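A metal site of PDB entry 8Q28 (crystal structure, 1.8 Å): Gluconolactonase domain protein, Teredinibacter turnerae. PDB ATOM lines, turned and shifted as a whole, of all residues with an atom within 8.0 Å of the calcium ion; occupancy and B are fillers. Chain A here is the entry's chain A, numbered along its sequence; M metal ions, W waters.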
ATOM      1  N   ASP A   9      16.845   5.091  23.046  1.00  0.00           N
ATOM      2  CA  ASP A   9      16.845   4.041  24.069  1.00  0.00           C
ATOM      3  C   ASP A   9      17.235   2.703  23.433  1.00  0.00           C
ATOM      4  O   ASP A   9      16.622   2.290  22.465  1.00  0.00           O
ATOM      5  CB  ASP A   9      15.509   3.949  24.801  1.00  0.00           C
ATOM      6  CG  ASP A   9      15.623   3.251  26.147  1.00  0.00           C
ATOM      7  OD1 ASP A   9      16.700   2.597  26.409  1.00  0.00           O
ATOM      8  OD2 ASP A   9      14.631   3.356  26.934  1.00  0.00           O
ATOM      9  N   GLY A  10      18.309   2.071  23.928  1.00  0.00           N
ATOM     10  CA  GLY A  10      18.822   0.776  23.499  1.00  0.00           C
ATOM     11  C   GLY A  10      18.457  -0.363  24.494  1.00  0.00           C
ATOM     12  O   GLY A  10      18.832  -1.517  24.314  1.00  0.00           O
ATOM     13  N   PHE A  11      17.830   0.033  25.587  1.00  0.00           N
ATOM     14  CA  PHE A  11      17.342  -0.845  26.655  1.00  0.00           C
ATOM     15  C   PHE A  11      18.457  -1.540  27.437  1.00  0.00           C
ATOM     16  O   PHE A  11      18.201  -2.522  28.137  1.00  0.00           O
ATOM     17  CB  PHE A  11      16.358  -1.850  26.069  1.00  0.00           C
ATOM     18  CG  PHE A  11      15.262  -1.112  25.341  1.00  0.00           C
ATOM     19  CD1 PHE A  11      14.289  -0.450  26.086  1.00  0.00           C
ATOM     20  CD2 PHE A  11      15.274  -1.006  23.970  1.00  0.00           C
ATOM     21  CE1 PHE A  11      13.335   0.320  25.420  1.00  0.00           C
ATOM     22  CE2 PHE A  11      14.284  -0.288  23.323  1.00  0.00           C
ATOM     23  CZ  PHE A  11      13.312   0.341  24.054  1.00  0.00           C
ATOM     24  N   GLU A  12      19.700  -1.061  27.330  1.00  0.00           N
ATOM     25  CA  GLU A  12      20.823  -1.801  27.880  1.00  0.00           C
ATOM     26  C   GLU A  12      20.845  -1.710  29.403  1.00  0.00           C
ATOM     27  O   GLU A  12      21.353  -2.620  30.031  1.00  0.00           O
ATOM     28  CB  GLU A  12      22.142  -1.370  27.258  1.00  0.00           C
ATOM     29  CG  GLU A  12      22.209  -1.601  25.794  1.00  0.00           C
ATOM     30  CD  GLU A  12      22.121  -3.068  25.453  1.00  0.00           C
ATOM     31  OE1 GLU A  12      22.861  -3.861  26.139  1.00  0.00           O
ATOM     32  OE2 GLU A  12      21.269  -3.439  24.562  1.00  0.00           O
ATOM     33  N   SER A  13      20.271  -0.660  29.994  1.00  0.00           N
ATOM     34  CA  SER A  13      20.357  -0.454  31.422  1.00  0.00           C
ATOM     35  C   SER A  13      19.212  -1.105  32.217  1.00  0.00           C
ATOM     36  O   SER A  13      19.295  -1.182  33.438  1.00  0.00           O
ATOM     37  CB  SER A  13      20.418   1.006  31.710  1.00  0.00           C
ATOM     38  OG  SER A  13      19.189   1.581  31.360  1.00  0.00           O
ATOM     39  N   ASP A  47      14.371  -7.960  26.920  1.00  0.00           N
ATOM     40  CA  ASP A  47      14.716  -9.325  26.623  1.00  0.00           C
ATOM     41  C   ASP A  47      16.181  -9.308  26.144  1.00  0.00           C
ATOM     42  O   ASP A  47      16.522  -8.581  25.225  1.00  0.00           O
ATOM     43  CB  ASP A  47      13.776  -9.840  25.541  1.00  0.00           C
ATOM     44  CG  ASP A  47      13.858 -11.296  25.073  1.00  0.00           C
ATOM     45  OD1 ASP A  47      14.823 -12.010  25.448  1.00  0.00           O
ATOM     46  OD2 ASP A  47      12.973 -11.669  24.277  1.00  0.00           O
ATOM     47  N   ARG A  50      17.540 -11.482  22.003  1.00  0.00           N
ATOM     48  CA  ARG A  50      17.606 -10.951  20.654  1.00  0.00           C
ATOM     49  C   ARG A  50      17.830  -9.450  20.807  1.00  0.00           C
ATOM     50  O   ARG A  50      17.357  -8.847  21.773  1.00  0.00           O
ATOM     51  CB  ARG A  50      16.313 -11.366  19.990  1.00  0.00           C
ATOM     52  CG  ARG A  50      16.040 -10.614  18.710  1.00  0.00           C
ATOM     53  CD  ARG A  50      14.903 -11.095  17.865  1.00  0.00           C
ATOM     54  NE  ARG A  50      15.263 -12.392  17.293  1.00  0.00           N
ATOM     55  CZ  ARG A  50      14.529 -13.471  17.395  1.00  0.00           C
ATOM     56  NH1 ARG A  50      13.381 -13.452  18.048  1.00  0.00           N
ATOM     57  NH2 ARG A  50      14.919 -14.591  16.790  1.00  0.00           N
ATOM     58  N   ALA A  51      18.664  -8.851  19.947  1.00  0.00           N
ATOM     59  CA  ALA A  51      18.991  -7.421  20.081  1.00  0.00           C
ATOM     60  C   ALA A  51      19.672  -6.982  18.792  1.00  0.00           C
ATOM     61  O   ALA A  51      20.169  -7.833  18.049  1.00  0.00           O
ATOM     62  CB  ALA A  51      19.836  -7.180  21.302  1.00  0.00           C
ATOM     63  N   PHE A  52      19.540  -5.695  18.420  1.00  0.00           N
ATOM     64  CA  PHE A  52      20.252  -5.219  17.248  1.00  0.00           C
ATOM     65  C   PHE A  52      21.609  -4.677  17.659  1.00  0.00           C
ATOM     66  O   PHE A  52      22.595  -4.772  16.892  1.00  0.00           O
ATOM     67  CB  PHE A  52      19.419  -4.187  16.483  1.00  0.00           C
ATOM     68  CG  PHE A  52      19.999  -3.924  15.140  1.00  0.00           C
ATOM     69  CD1 PHE A  52      19.852  -4.870  14.140  1.00  0.00           C
ATOM     70  CD2 PHE A  52      20.717  -2.768  14.873  1.00  0.00           C
ATOM     71  CE1 PHE A  52      20.387  -4.687  12.875  1.00  0.00           C
ATOM     72  CE2 PHE A  52      21.349  -2.613  13.660  1.00  0.00           C
ATOM     73  CZ  PHE A  52      21.135  -3.526  12.637  1.00  0.00           C
ATOM     74  N   THR A  53      21.647  -3.985  18.799  1.00  0.00           N
ATOM     75  CA  THR A  53      22.891  -3.495  19.356  1.00  0.00           C
ATOM     76  C   THR A  53      22.950  -3.862  20.825  1.00  0.00           C
ATOM     77  O   THR A  53      21.949  -3.695  21.556  1.00  0.00           O
ATOM     78  CB  THR A  53      23.001  -1.953  19.253  1.00  0.00           C
ATOM     79  OG1 THR A  53      22.589  -1.584  17.949  1.00  0.00           O
ATOM     80  CG2 THR A  53      24.397  -1.431  19.509  1.00  0.00           C
ATOM     81  N   GLY A  54      24.133  -4.283  21.286  1.00  0.00           N
ATOM     82  CA  GLY A  54      24.284  -4.631  22.687  1.00  0.00           C
ATOM     83  C   GLY A  54      23.549  -5.940  22.979  1.00  0.00           C
ATOM     84  O   GLY A  54      23.380  -6.746  22.057  1.00  0.00           O
ATOM     85  N   ASN A  55      23.157  -6.142  24.242  1.00  0.00           N
ATOM     86  CA  ASN A  55      22.542  -7.407  24.666  1.00  0.00           C
ATOM     87  C   ASN A  55      21.015  -7.371  24.659  1.00  0.00           C
ATOM     88  O   ASN A  55      20.390  -8.429  24.551  1.00  0.00           O
ATOM     89  CB  ASN A  55      23.030  -7.690  26.056  1.00  0.00           C
ATOM     90  CG  ASN A  55      24.538  -7.910  25.962  1.00  0.00           C
ATOM     91  OD1 ASN A  55      25.019  -8.637  25.109  1.00  0.00           O
ATOM     92  ND2 ASN A  55      25.273  -7.275  26.811  1.00  0.00           N
ATOM     93  N   ASN A  56      20.438  -6.202  24.755  1.00  0.00           N
ATOM     94  CA  ASN A  56      19.014  -6.189  25.117  1.00  0.00           C
ATOM     95  C   ASN A  56      18.134  -5.568  24.033  1.00  0.00           C
ATOM     96  O   ASN A  56      18.506  -4.643  23.326  1.00  0.00           O
ATOM     97  CB  ASN A  56      18.773  -5.390  26.383  1.00  0.00           C
ATOM     98  CG  ASN A  56      19.324  -6.028  27.629  1.00  0.00           C
ATOM     99  OD1 ASN A  56      19.678  -7.189  27.607  1.00  0.00           O
ATOM    100  ND2 ASN A  56      19.358  -5.270  28.697  1.00  0.00           N
ATOM    101  N   SER A  57      16.886  -5.974  24.002  1.00  0.00           N
ATOM    102  CA  SER A  57      15.875  -5.285  23.243  1.00  0.00           C
ATOM    103  C   SER A  57      14.650  -5.206  24.154  1.00  0.00           C
ATOM    104  O   SER A  57      14.649  -5.797  25.210  1.00  0.00           O
ATOM    105  CB  SER A  57      15.536  -6.081  21.973  1.00  0.00           C
ATOM    106  OG  SER A  57      15.073  -7.402  22.271  1.00  0.00           O
ATOM    107  N   VAL A  58      13.593  -4.596  23.634  1.00  0.00           N
ATOM    108  CA  VAL A  58      12.270  -4.774  24.225  1.00  0.00           C
ATOM    109  C   VAL A  58      11.467  -5.799  23.394  1.00  0.00           C
ATOM    110  O   VAL A  58      11.335  -5.686  22.144  1.00  0.00           O
ATOM    111  CB  VAL A  58      11.539  -3.430  24.375  1.00  0.00           C
ATOM    112  CG1 VAL A  58      11.377  -2.677  23.047  1.00  0.00           C
ATOM    113  CG2 VAL A  58      10.168  -3.661  25.050  1.00  0.00           C
ATOM    114  N   TRP A 154      15.653  -7.963  10.845  1.00  0.00           N
ATOM    115  CA  TRP A 154      15.678  -6.655  11.486  1.00  0.00           C
ATOM    116  C   TRP A 154      15.441  -5.592  10.437  1.00  0.00           C
ATOM    117  O   TRP A 154      15.985  -5.702   9.354  1.00  0.00           O
ATOM    118  CB  TRP A 154      17.014  -6.417  12.180  1.00  0.00           C
ATOM    119  CG  TRP A 154      17.195  -7.070  13.495  1.00  0.00           C
ATOM    120  CD1 TRP A 154      17.972  -8.149  13.769  1.00  0.00           C
ATOM    121  CD2 TRP A 154      16.607  -6.628  14.734  1.00  0.00           C
ATOM    122  NE1 TRP A 154      17.960  -8.410  15.115  1.00  0.00           N
ATOM    123  CE2 TRP A 154      17.088  -7.509  15.720  1.00  0.00           C
ATOM    124  CE3 TRP A 154      15.680  -5.598  15.084  1.00  0.00           C
ATOM    125  CZ2 TRP A 154      16.674  -7.397  17.037  1.00  0.00           C
ATOM    126  CZ3 TRP A 154      15.359  -5.481  16.392  1.00  0.00           C
ATOM    127  CH2 TRP A 154      15.791  -6.390  17.345  1.00  0.00           C
ATOM    128  N   MET A 224      12.064  -4.720  19.512  1.00  0.00           N
ATOM    129  CA  MET A 224      12.609  -3.486  18.987  1.00  0.00           C
ATOM    130  C   MET A 224      13.824  -3.148  19.794  1.00  0.00           C
ATOM    131  O   MET A 224      13.970  -3.553  20.951  1.00  0.00           O
ATOM    132  CB  MET A 224      11.531  -2.410  19.034  1.00  0.00           C
ATOM    133  CG  MET A 224      10.322  -2.667  18.329  1.00  0.00           C
ATOM    134  SD  MET A 224       9.145  -1.060  18.152  1.00  0.00           S
ATOM    135  CE  MET A 224       7.518  -1.869  17.511  1.00  0.00           C
ATOM    136  N   ASP A 225      14.674  -2.324  19.180  1.00  0.00           N
ATOM    137  CA  ASP A 225      15.901  -1.832  19.751  1.00  0.00           C
ATOM    138  C   ASP A 225      16.230  -0.460  19.106  1.00  0.00           C
ATOM    139  O   ASP A 225      15.700  -0.057  18.049  1.00  0.00           O
ATOM    140  CB  ASP A 225      17.003  -2.876  19.503  1.00  0.00           C
ATOM    141  CG  ASP A 225      18.188  -2.741  20.424  1.00  0.00           C
ATOM    142  OD1 ASP A 225      18.086  -1.942  21.427  1.00  0.00           O
ATOM    143  OD2 ASP A 225      19.161  -3.573  20.297  1.00  0.00           O
ATOM    144  N   ASP A 226      17.050   0.273  19.819  1.00  0.00           N
ATOM    145  CA  ASP A 226      17.557   1.552  19.368  1.00  0.00           C
ATOM    146  C   ASP A 226      16.420   2.448  18.933  1.00  0.00           C
ATOM    147  O   ASP A 226      16.339   2.924  17.788  1.00  0.00           O
ATOM    148  CB  ASP A 226      18.599   1.317  18.267  1.00  0.00           C
ATOM    149  CG  ASP A 226      19.704   0.373  18.706  1.00  0.00           C
ATOM    150  OD1 ASP A 226      20.110   0.535  19.843  1.00  0.00           O
ATOM    151  OD2 ASP A 226      20.087  -0.544  17.870  1.00  0.00           O
ATOM    152  N   ILE A 227      15.446   2.576  19.823  1.00  0.00           N
ATOM    153  CA  ILE A 227      14.291   3.417  19.530  1.00  0.00           C
ATOM    154  C   ILE A 227      14.701   4.877  19.640  1.00  0.00           C
ATOM    155  O   ILE A 227      15.433   5.231  20.579  1.00  0.00           O
ATOM    156  CB  ILE A 227      13.126   3.061  20.468  1.00  0.00           C
ATOM    157  CG1 ILE A 227      12.682   1.617  20.228  1.00  0.00           C
ATOM    158  CG2 ILE A 227      12.035   4.058  20.262  1.00  0.00           C
ATOM    159  CD1 ILE A 227      11.378   1.160  20.977  1.00  0.00           C
HETATM  160 CA    CA M   1      20.013  -2.823  22.684  1.00  0.00          CA
HETATM  161  O   HOH W   1      21.168  -0.875  21.992  1.00  0.00           O
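The side-chain carboxylate of Glu 12 sits at hydrogen-bond distance from the backbone NH of Asn 55, 3.0 Å away.
The side-chain carboxylate (OD2) of Asp 226 sits at hydrogen-bond distance from the side-chain hydroxyl (OG1) of Thr 53 (2.7 Å).
ND2 of Asn 56 lies within hydrogen-bond range of O of Phe 11, at 3.0 Å.
N of Phe 52 sits close to OD2 of Asp 225 (2.9 Å).
Within 4 Å of the calcium ion: Gly 10, Glu 12, Thr 53, Asn 56 and Asp 225.
Along chain A the residues within 4 Å of the calcium ion span positions 10 to 225.
The nearest printed residue that does not touch the calcium ion is Asp 226 (4.4 Å).
The calcium ion is bound by OE2 of Glu 12 (2.3 Å), water W1 (2.4 Å), O of Gly 10 (2.4 Å), O of Thr 53 (2.4 Å), O of Asn 56 (2.4 Å), OD1 of Asp 225 (2.5 Å) and OD2 of Asp 225 (2.6 Å).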
